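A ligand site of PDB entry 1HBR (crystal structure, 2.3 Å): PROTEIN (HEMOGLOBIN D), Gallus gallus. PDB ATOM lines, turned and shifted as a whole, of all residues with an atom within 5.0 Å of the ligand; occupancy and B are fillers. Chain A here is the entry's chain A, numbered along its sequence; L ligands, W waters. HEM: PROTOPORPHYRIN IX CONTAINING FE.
NE2 of His 87 binds FE of the ligand (2.1 Å). An oxygen (O1D) of the ligand sits at hydrogen-bond distance from a ring nitrogen (NE2) of His 45, at 2.7 Å. An oxygen (O1A) of the ligand is in salt-bridge range of the side-chain amino group of Lys 61.
O of His 87 sits at hydrogen-bond distance from N of Val 93, at 3.0 Å. ND1 of His 87 sits at hydrogen-bond distance from O of Leu 83 (2.7 Å). The side-chain hydroxyl (OH) of Tyr 42 lies within hydrogen-bond range of the side-chain amide oxygen (OD1) of Asn 97 (3.4 Å). The backbone NH (N) of Leu 91 lies within hydrogen-bond range of the backbone carbonyl oxygen (O) of Leu 86, 2.8 Å away.
Tyr 42 touches the ligand (O to CMD, 3.2 Å). CE1 of Phe 43 touches CMD of the ligand, 3.5 Å away. CE1 of Phe 46 touches O1D of the ligand, 3.6 Å away. His 58 touches the ligand. Ala 65 touches the ligand (CB to CMB, 3.98 Å). CD2 of Leu 83 touches CMA of the ligand, at 3.6 Å. Leu 86 touches the ligand. Leu 91 touches the ligand (CD1 to C3D, 3.5 Å). Val 93 touches the ligand (CG1 to CAC, 3.5 Å). Asn 97 touches the ligand. CE1 of Phe 98 touches CHC of the ligand, 3.7 Å away. CD2 of Leu 101 touches CHC of the ligand (3.5 Å). CD1 of Leu 136 touches C3B of the ligand (3.7 Å). Hydrophobic or aromatic side chains within 4 Å of the ligand: Tyr 42, Phe 43, His 45, Phe 46, His 58, Ala 65, Leu 83, Leu 86, His 87, Leu 91, Val 93, Phe 98, Leu 101 and Leu 136. 16 residues have an atom within 4 Å of the ligand: Tyr 42, Phe 43, His 45, Phe 46, His 58, Lys 61, Ala 65, Leu 83, Leu 86, His 87, Leu 91, Val 93, Asn 97, Phe 98, Leu 101 and Leu 136. The nearest printed residue that does not touch the ligand is Met 80 (4.1 Å).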
ATOM      1  N   MET A  32       4.105   6.813  -8.596  1.00  0.00           N
ATOM      2  CA  MET A  32       3.223   7.493  -9.534  1.00  0.00           C
ATOM      3  C   MET A  32       2.343   8.507  -8.807  1.00  0.00           C
ATOM      4  O   MET A  32       2.348   9.693  -9.151  1.00  0.00           O
ATOM      5  CB  MET A  32       2.360   6.488 -10.306  1.00  0.00           C
ATOM      6  CG  MET A  32       1.359   7.143 -11.251  1.00  0.00           C
ATOM      7  SD  MET A  32       0.480   6.004 -12.316  1.00  0.00           S
ATOM      8  CE  MET A  32      -0.614   5.205 -11.157  1.00  0.00           C
ATOM      9  N   THR A  39      -2.897  11.531 -11.030  1.00  0.00           N
ATOM     10  CA  THR A  39      -3.319  10.136 -11.212  1.00  0.00           C
ATOM     11  C   THR A  39      -4.235   9.611 -10.094  1.00  0.00           C
ATOM     12  O   THR A  39      -5.003   8.678 -10.299  1.00  0.00           O
ATOM     13  CB  THR A  39      -2.108   9.196 -11.378  1.00  0.00           C
ATOM     14  OG1 THR A  39      -1.182   9.397 -10.306  1.00  0.00           O
ATOM     15  CG2 THR A  39      -1.399   9.456 -12.703  1.00  0.00           C
ATOM     16  N   TYR A  42      -8.028   8.699 -10.461  1.00  0.00           N
ATOM     17  CA  TYR A  42      -8.585   7.431 -10.908  1.00  0.00           C
ATOM     18  C   TYR A  42      -8.894   6.446  -9.792  1.00  0.00           C
ATOM     19  O   TYR A  42      -9.568   5.429 -10.008  1.00  0.00           O
ATOM     20  CB  TYR A  42      -7.664   6.772 -11.926  1.00  0.00           C
ATOM     21  CG  TYR A  42      -7.635   7.489 -13.243  1.00  0.00           C
ATOM     22  CD1 TYR A  42      -6.851   8.627 -13.426  1.00  0.00           C
ATOM     23  CD2 TYR A  42      -8.409   7.044 -14.325  1.00  0.00           C
ATOM     24  CE1 TYR A  42      -6.830   9.297 -14.641  1.00  0.00           C
ATOM     25  CE2 TYR A  42      -8.388   7.714 -15.541  1.00  0.00           C
ATOM     26  CZ  TYR A  42      -7.599   8.841 -15.692  1.00  0.00           C
ATOM     27  OH  TYR A  42      -7.560   9.501 -16.898  1.00  0.00           O
ATOM     28  N   PHE A  43      -8.408   6.751  -8.590  1.00  0.00           N
ATOM     29  CA  PHE A  43      -8.624   5.871  -7.453  1.00  0.00           C
ATOM     30  C   PHE A  43      -9.307   6.629  -6.299  1.00  0.00           C
ATOM     31  O   PHE A  43      -8.783   6.662  -5.177  1.00  0.00           O
ATOM     32  CB  PHE A  43      -7.283   5.276  -6.993  1.00  0.00           C
ATOM     33  CG  PHE A  43      -6.534   4.523  -8.066  1.00  0.00           C
ATOM     34  CD1 PHE A  43      -6.752   3.157  -8.267  1.00  0.00           C
ATOM     35  CD2 PHE A  43      -5.597   5.162  -8.866  1.00  0.00           C
ATOM     36  CE1 PHE A  43      -6.022   2.452  -9.213  1.00  0.00           C
ATOM     37  CE2 PHE A  43      -4.865   4.462  -9.820  1.00  0.00           C
ATOM     38  CZ  PHE A  43      -5.084   3.102  -9.992  1.00  0.00           C
ATOM     39  N   HIS A  45     -11.801   5.679  -4.632  1.00  0.00           N
ATOM     40  CA  HIS A  45     -12.239   4.658  -3.694  1.00  0.00           C
ATOM     41  C   HIS A  45     -11.094   4.052  -2.866  1.00  0.00           C
ATOM     42  O   HIS A  45     -11.329   3.290  -1.937  1.00  0.00           O
ATOM     43  CB  HIS A  45     -12.987   3.524  -4.453  1.00  0.00           C
ATOM     44  CG  HIS A  45     -12.235   2.973  -5.633  1.00  0.00           C
ATOM     45  ND1 HIS A  45     -11.421   3.753  -6.427  1.00  0.00           N
ATOM     46  CD2 HIS A  45     -12.176   1.726  -6.145  1.00  0.00           C
ATOM     47  CE1 HIS A  45     -10.878   2.998  -7.364  1.00  0.00           C
ATOM     48  NE2 HIS A  45     -11.319   1.771  -7.225  1.00  0.00           N
ATOM     49  N   PHE A  46      -9.851   4.313  -3.286  1.00  0.00           N
ATOM     50  CA  PHE A  46      -8.677   3.789  -2.593  1.00  0.00           C
ATOM     51  C   PHE A  46      -8.182   4.662  -1.454  1.00  0.00           C
ATOM     52  O   PHE A  46      -8.374   5.873  -1.444  1.00  0.00           O
ATOM     53  CB  PHE A  46      -7.499   3.702  -3.564  1.00  0.00           C
ATOM     54  CG  PHE A  46      -7.391   2.407  -4.296  1.00  0.00           C
ATOM     55  CD1 PHE A  46      -8.525   1.708  -4.672  1.00  0.00           C
ATOM     56  CD2 PHE A  46      -6.149   1.907  -4.646  1.00  0.00           C
ATOM     57  CE1 PHE A  46      -8.434   0.532  -5.374  1.00  0.00           C
ATOM     58  CE2 PHE A  46      -6.037   0.732  -5.355  1.00  0.00           C
ATOM     59  CZ  PHE A  46      -7.189   0.046  -5.727  1.00  0.00           C
ATOM     60  N   HIS A  58      -3.253  -3.745  -5.018  1.00  0.00           N
ATOM     61  CA  HIS A  58      -3.359  -3.384  -6.414  1.00  0.00           C
ATOM     62  C   HIS A  58      -2.014  -3.587  -7.093  1.00  0.00           C
ATOM     63  O   HIS A  58      -1.939  -4.221  -8.143  1.00  0.00           O
ATOM     64  CB  HIS A  58      -3.814  -1.941  -6.578  1.00  0.00           C
ATOM     65  CG  HIS A  58      -4.266  -1.607  -7.963  1.00  0.00           C
ATOM     66  ND1 HIS A  58      -5.039  -2.474  -8.704  1.00  0.00           N
ATOM     67  CD2 HIS A  58      -4.017  -0.547  -8.756  1.00  0.00           C
ATOM     68  CE1 HIS A  58      -5.248  -1.954  -9.903  1.00  0.00           C
ATOM     69  NE2 HIS A  58      -4.633  -0.791  -9.960  1.00  0.00           N
ATOM     70  N   LYS A  61      -1.452  -6.855  -8.236  1.00  0.00           N
ATOM     71  CA  LYS A  61      -2.260  -7.244  -9.386  1.00  0.00           C
ATOM     72  C   LYS A  61      -1.651  -6.682 -10.674  1.00  0.00           C
ATOM     73  O   LYS A  61      -1.637  -7.356 -11.705  1.00  0.00           O
ATOM     74  CB  LYS A  61      -3.709  -6.768  -9.212  1.00  0.00           C
ATOM     75  CG  LYS A  61      -4.514  -7.630  -8.239  1.00  0.00           C
ATOM     76  CD  LYS A  61      -5.590  -6.849  -7.507  1.00  0.00           C
ATOM     77  CE  LYS A  61      -6.717  -6.466  -8.410  1.00  0.00           C
ATOM     78  NZ  LYS A  61      -7.592  -5.429  -7.801  1.00  0.00           N
ATOM     79  N   VAL A  62      -1.127  -5.459 -10.587  1.00  0.00           N
ATOM     80  CA  VAL A  62      -0.497  -4.796 -11.726  1.00  0.00           C
ATOM     81  C   VAL A  62       0.717  -5.604 -12.197  1.00  0.00           C
ATOM     82  O   VAL A  62       0.777  -6.023 -13.349  1.00  0.00           O
ATOM     83  CB  VAL A  62      -0.039  -3.357 -11.357  1.00  0.00           C
ATOM     84  CG1 VAL A  62       0.756  -2.731 -12.483  1.00  0.00           C
ATOM     85  CG2 VAL A  62      -1.251  -2.499 -11.025  1.00  0.00           C
ATOM     86  N   ALA A  65      -0.072  -8.853 -13.879  1.00  0.00           N
ATOM     87  CA  ALA A  65      -0.490  -8.691 -15.275  1.00  0.00           C
ATOM     88  C   ALA A  65       0.731  -8.574 -16.195  1.00  0.00           C
ATOM     89  O   ALA A  65       0.772  -9.179 -17.258  1.00  0.00           O
ATOM     90  CB  ALA A  65      -1.365  -7.461 -15.411  1.00  0.00           C
ATOM     91  N   LEU A  66       1.699  -7.769 -15.772  1.00  0.00           N
ATOM     92  CA  LEU A  66       2.924  -7.576 -16.539  1.00  0.00           C
ATOM     93  C   LEU A  66       3.647  -8.909 -16.707  1.00  0.00           C
ATOM     94  O   LEU A  66       4.167  -9.219 -17.788  1.00  0.00           O
ATOM     95  CB  LEU A  66       3.836  -6.567 -15.853  1.00  0.00           C
ATOM     96  CG  LEU A  66       3.382  -5.116 -16.011  1.00  0.00           C
ATOM     97  CD1 LEU A  66       4.312  -4.222 -15.239  1.00  0.00           C
ATOM     98  CD2 LEU A  66       3.368  -4.739 -17.485  1.00  0.00           C
ATOM     99  N   MET A  80      -4.035  -9.213 -23.058  1.00  0.00           N
ATOM    100  CA  MET A  80      -4.417  -8.002 -22.338  1.00  0.00           C
ATOM    101  C   MET A  80      -5.823  -7.537 -22.742  1.00  0.00           C
ATOM    102  O   MET A  80      -6.275  -6.467 -22.309  1.00  0.00           O
ATOM    103  CB  MET A  80      -3.421  -6.877 -22.652  1.00  0.00           C
ATOM    104  CG  MET A  80      -1.943  -7.219 -22.418  1.00  0.00           C
ATOM    105  SD  MET A  80      -1.487  -7.365 -20.692  1.00  0.00           S
ATOM    106  CE  MET A  80      -1.422  -5.623 -20.219  1.00  0.00           C
ATOM    107  N   LEU A  83      -8.097  -6.347 -20.018  1.00  0.00           N
ATOM    108  CA  LEU A  83      -7.555  -5.140 -19.418  1.00  0.00           C
ATOM    109  C   LEU A  83      -7.722  -3.894 -20.268  1.00  0.00           C
ATOM    110  O   LEU A  83      -7.946  -2.816 -19.726  1.00  0.00           O
ATOM    111  CB  LEU A  83      -6.096  -5.371 -19.038  1.00  0.00           C
ATOM    112  CG  LEU A  83      -5.881  -6.272 -17.815  1.00  0.00           C
ATOM    113  CD1 LEU A  83      -4.392  -6.412 -17.550  1.00  0.00           C
ATOM    114  CD2 LEU A  83      -6.586  -5.685 -16.610  1.00  0.00           C
ATOM    115  N   LEU A  86     -11.290  -2.773 -19.948  1.00  0.00           N
ATOM    116  CA  LEU A  86     -11.529  -2.141 -18.653  1.00  0.00           C
ATOM    117  C   LEU A  86     -10.994  -0.714 -18.645  1.00  0.00           C
ATOM    118  O   LEU A  86     -11.722   0.234 -18.323  1.00  0.00           O
ATOM    119  CB  LEU A  86     -10.844  -2.949 -17.528  1.00  0.00           C
ATOM    120  CG  LEU A  86     -11.297  -2.842 -16.064  1.00  0.00           C
ATOM    121  CD1 LEU A  86     -10.103  -3.165 -15.190  1.00  0.00           C
ATOM    122  CD2 LEU A  86     -11.829  -1.475 -15.729  1.00  0.00           C
ATOM    123  N   HIS A  87      -9.720  -0.567 -19.000  1.00  0.00           N
ATOM    124  CA  HIS A  87      -9.059   0.736 -18.986  1.00  0.00           C
ATOM    125  C   HIS A  87      -9.587   1.730 -20.008  1.00  0.00           C
ATOM    126  O   HIS A  87      -9.792   2.908 -19.676  1.00  0.00           O
ATOM    127  CB  HIS A  87      -7.546   0.560 -19.123  1.00  0.00           C
ATOM    128  CG  HIS A  87      -6.896  -0.058 -17.925  1.00  0.00           C
ATOM    129  ND1 HIS A  87      -6.829  -1.433 -17.732  1.00  0.00           N
ATOM    130  CD2 HIS A  87      -6.303   0.498 -16.835  1.00  0.00           C
ATOM    131  CE1 HIS A  87      -6.237  -1.684 -16.579  1.00  0.00           C
ATOM    132  NE2 HIS A  87      -5.913  -0.543 -16.026  1.00  0.00           N
ATOM    133  N   LEU A  91     -13.069   2.546 -17.626  1.00  0.00           N
ATOM    134  CA  LEU A  91     -12.375   3.605 -16.907  1.00  0.00           C
ATOM    135  C   LEU A  91     -12.070   4.889 -17.645  1.00  0.00           C
ATOM    136  O   LEU A  91     -11.954   5.952 -17.022  1.00  0.00           O
ATOM    137  CB  LEU A  91     -11.077   3.046 -16.333  1.00  0.00           C
ATOM    138  CG  LEU A  91     -11.257   1.918 -15.309  1.00  0.00           C
ATOM    139  CD1 LEU A  91      -9.945   1.205 -15.073  1.00  0.00           C
ATOM    140  CD2 LEU A  91     -11.828   2.488 -14.024  1.00  0.00           C
ATOM    141  N   VAL A  93      -9.243   5.755 -19.083  1.00  0.00           N
ATOM    142  CA  VAL A  93      -7.943   6.257 -18.630  1.00  0.00           C
ATOM    143  C   VAL A  93      -7.262   7.014 -19.755  1.00  0.00           C
ATOM    144  O   VAL A  93      -7.079   6.480 -20.846  1.00  0.00           O
ATOM    145  CB  VAL A  93      -6.978   5.121 -18.197  1.00  0.00           C
ATOM    146  CG1 VAL A  93      -5.672   5.722 -17.675  1.00  0.00           C
ATOM    147  CG2 VAL A  93      -7.613   4.213 -17.166  1.00  0.00           C
ATOM    148  N   ASN A  97      -1.353   8.750 -19.115  1.00  0.00           N
ATOM    149  CA  ASN A  97      -1.055   8.102 -17.847  1.00  0.00           C
ATOM    150  C   ASN A  97      -0.282   6.792 -17.938  1.00  0.00           C
ATOM    151  O   ASN A  97       0.460   6.445 -17.014  1.00  0.00           O
ATOM    152  CB  ASN A  97      -2.331   7.930 -17.028  1.00  0.00           C
ATOM    153  CG  ASN A  97      -2.978   9.255 -16.662  1.00  0.00           C
ATOM    154  OD1 ASN A  97      -4.173   9.447 -16.859  1.00  0.00           O
ATOM    155  ND2 ASN A  97      -2.184  10.181 -16.160  1.00  0.00           N
ATOM    156  N   PHE A  98      -0.453   6.055 -19.030  1.00  0.00           N
ATOM    157  CA  PHE A  98       0.275   4.795 -19.196  1.00  0.00           C
ATOM    158  C   PHE A  98       1.772   5.080 -19.243  1.00  0.00           C
ATOM    159  O   PHE A  98       2.571   4.277 -18.768  1.00  0.00           O
ATOM    160  CB  PHE A  98      -0.170   4.060 -20.451  1.00  0.00           C
ATOM    161  CG  PHE A  98      -1.555   3.504 -20.366  1.00  0.00           C
ATOM    162  CD1 PHE A  98      -1.849   2.461 -19.484  1.00  0.00           C
ATOM    163  CD2 PHE A  98      -2.569   4.020 -21.152  1.00  0.00           C
ATOM    164  CE1 PHE A  98      -3.132   1.949 -19.396  1.00  0.00           C
ATOM    165  CE2 PHE A  98      -3.860   3.515 -21.072  1.00  0.00           C
ATOM    166  CZ  PHE A  98      -4.141   2.483 -20.192  1.00  0.00           C
ATOM    167  N   LEU A 101       2.947   5.534 -15.575  1.00  0.00           N
ATOM    168  CA  LEU A 101       3.155   4.300 -14.818  1.00  0.00           C
ATOM    169  C   LEU A 101       4.426   3.600 -15.312  1.00  0.00           C
ATOM    170  O   LEU A 101       5.250   3.163 -14.505  1.00  0.00           O
ATOM    171  CB  LEU A 101       1.936   3.365 -14.920  1.00  0.00           C
ATOM    172  CG  LEU A 101       1.984   2.102 -14.035  1.00  0.00           C
ATOM    173  CD1 LEU A 101       2.303   2.477 -12.601  1.00  0.00           C
ATOM    174  CD2 LEU A 101       0.685   1.333 -14.090  1.00  0.00           C
ATOM    175  N   VAL A 132       2.951  -2.698 -24.291  1.00  0.00           N
ATOM    176  CA  VAL A 132       1.875  -3.041 -23.369  1.00  0.00           C
ATOM    177  C   VAL A 132       0.901  -1.871 -23.211  1.00  0.00           C
ATOM    178  O   VAL A 132      -0.314  -2.058 -23.192  1.00  0.00           O
ATOM    179  CB  VAL A 132       2.464  -3.408 -21.987  1.00  0.00           C
ATOM    180  CG1 VAL A 132       1.377  -3.430 -20.921  1.00  0.00           C
ATOM    181  CG2 VAL A 132       3.141  -4.763 -22.045  1.00  0.00           C
ATOM    182  N   SER A 133       1.454  -0.665 -23.141  1.00  0.00           N
ATOM    183  CA  SER A 133       0.656   0.546 -23.013  1.00  0.00           C
ATOM    184  C   SER A 133      -0.225   0.767 -24.230  1.00  0.00           C
ATOM    185  O   SER A 133      -1.355   1.221 -24.132  1.00  0.00           O
ATOM    186  CB  SER A 133       1.571   1.758 -22.829  1.00  0.00           C
ATOM    187  OG  SER A 133       2.265   1.717 -21.594  1.00  0.00           O
ATOM    188  N   LEU A 136      -3.285  -1.407 -24.317  1.00  0.00           N
ATOM    189  CA  LEU A 136      -4.253  -1.042 -23.278  1.00  0.00           C
ATOM    190  C   LEU A 136      -5.143   0.106 -23.710  1.00  0.00           C
ATOM    191  O   LEU A 136      -6.243   0.293 -23.183  1.00  0.00           O
ATOM    192  CB  LEU A 136      -3.545  -0.719 -21.963  1.00  0.00           C
ATOM    193  CG  LEU A 136      -3.013  -1.916 -21.178  1.00  0.00           C
ATOM    194  CD1 LEU A 136      -2.633  -1.507 -19.769  1.00  0.00           C
ATOM    195  CD2 LEU A 136      -4.104  -2.958 -21.126  1.00  0.00           C
HETATM  196  CHA HEM L   1      -7.367  -1.897 -12.686  1.00  0.00           C
HETATM  197  CHB HEM L   1      -3.294  -3.477 -14.701  1.00  0.00           C
HETATM  198  CHC HEM L   1      -2.218   1.024 -15.935  1.00  0.00           C
HETATM  199  CHD HEM L   1      -5.930   2.628 -13.349  1.00  0.00           C
HETATM  200  C1A HEM L   1      -6.297  -2.711 -13.046  1.00  0.00           C
HETATM  201  C2A HEM L   1      -6.282  -4.132 -12.846  1.00  0.00           C
HETATM  202  C3A HEM L   1      -5.142  -4.570 -13.413  1.00  0.00           C
HETATM  203  C4A HEM L   1      -4.432  -3.404 -13.890  1.00  0.00           C
HETATM  204  CMA HEM L   1      -4.694  -6.019 -13.565  1.00  0.00           C
HETATM  205  CAA HEM L   1      -7.271  -4.887 -11.978  1.00  0.00           C
HETATM  206  CBA HEM L   1      -8.136  -5.953 -12.631  1.00  0.00           C
HETATM  207  CGA HEM L   1      -9.301  -6.394 -11.761  1.00  0.00           C
HETATM  208  O1A HEM L   1      -9.131  -6.478 -10.517  1.00  0.00           O
HETATM  209  O2A HEM L   1     -10.389  -6.632 -12.316  1.00  0.00           O
HETATM  210  C1B HEM L   1      -2.684  -2.387 -15.291  1.00  0.00           C
HETATM  211  C2B HEM L   1      -1.474  -2.464 -16.112  1.00  0.00           C
HETATM  212  C3B HEM L   1      -1.098  -1.199 -16.376  1.00  0.00           C
HETATM  213  C4B HEM L   1      -2.184  -0.353 -15.850  1.00  0.00           C
HETATM  214  CMB HEM L   1      -0.797  -3.727 -16.675  1.00  0.00           C
HETATM  215  CAB HEM L   1       0.178  -0.829 -16.763  1.00  0.00           C
HETATM  216  CBB HEM L   1       0.522  -0.310 -18.069  1.00  0.00           C
HETATM  217  C1C HEM L   1      -3.084   1.852 -15.246  1.00  0.00           C
HETATM  218  C2C HEM L   1      -2.986   3.300 -15.252  1.00  0.00           C
HETATM  219  C3C HEM L   1      -4.090   3.744 -14.598  1.00  0.00           C
HETATM  220  C4C HEM L   1      -4.792   2.570 -14.112  1.00  0.00           C
HETATM  221  CMC HEM L   1      -1.857   4.149 -15.800  1.00  0.00           C
HETATM  222  CAC HEM L   1      -4.549   5.045 -14.464  1.00  0.00           C
HETATM  223  CBC HEM L   1      -3.799   6.130 -13.863  1.00  0.00           C
HETATM  224  C1D HEM L   1      -6.632   1.538 -12.892  1.00  0.00           C
HETATM  225  C2D HEM L   1      -7.901   1.592 -12.163  1.00  0.00           C
HETATM  226  C3D HEM L   1      -8.323   0.325 -12.109  1.00  0.00           C
HETATM  227  C4D HEM L   1      -7.340  -0.514 -12.741  1.00  0.00           C
HETATM  228  CMD HEM L   1      -8.602   2.780 -11.509  1.00  0.00           C
HETATM  229  CAD HEM L   1      -9.556  -0.144 -11.372  1.00  0.00           C
HETATM  230  CBD HEM L   1      -9.190  -0.524  -9.940  1.00  0.00           C
HETATM  231  CGD HEM L   1     -10.360  -1.068  -9.167  1.00  0.00           C
HETATM  232  O1D HEM L   1     -10.538  -0.663  -8.002  1.00  0.00           O
HETATM  233  O2D HEM L   1     -11.110  -1.899  -9.705  1.00  0.00           O
HETATM  234  NA  HEM L   1      -5.138  -2.246 -13.641  1.00  0.00           N
HETATM  235  NB  HEM L   1      -3.122  -1.082 -15.150  1.00  0.00           N
HETATM  236  NC  HEM L   1      -4.168   1.407 -14.508  1.00  0.00           N
HETATM  237  ND  HEM L   1      -6.282   0.231 -13.216  1.00  0.00           N
HETATM  238 FE   HEM L   1      -4.779  -0.411 -14.271  1.00  0.00          FE
HETATM  239  O   HOH W   1     -11.019  -4.173 -11.436  1.00  0.00           O
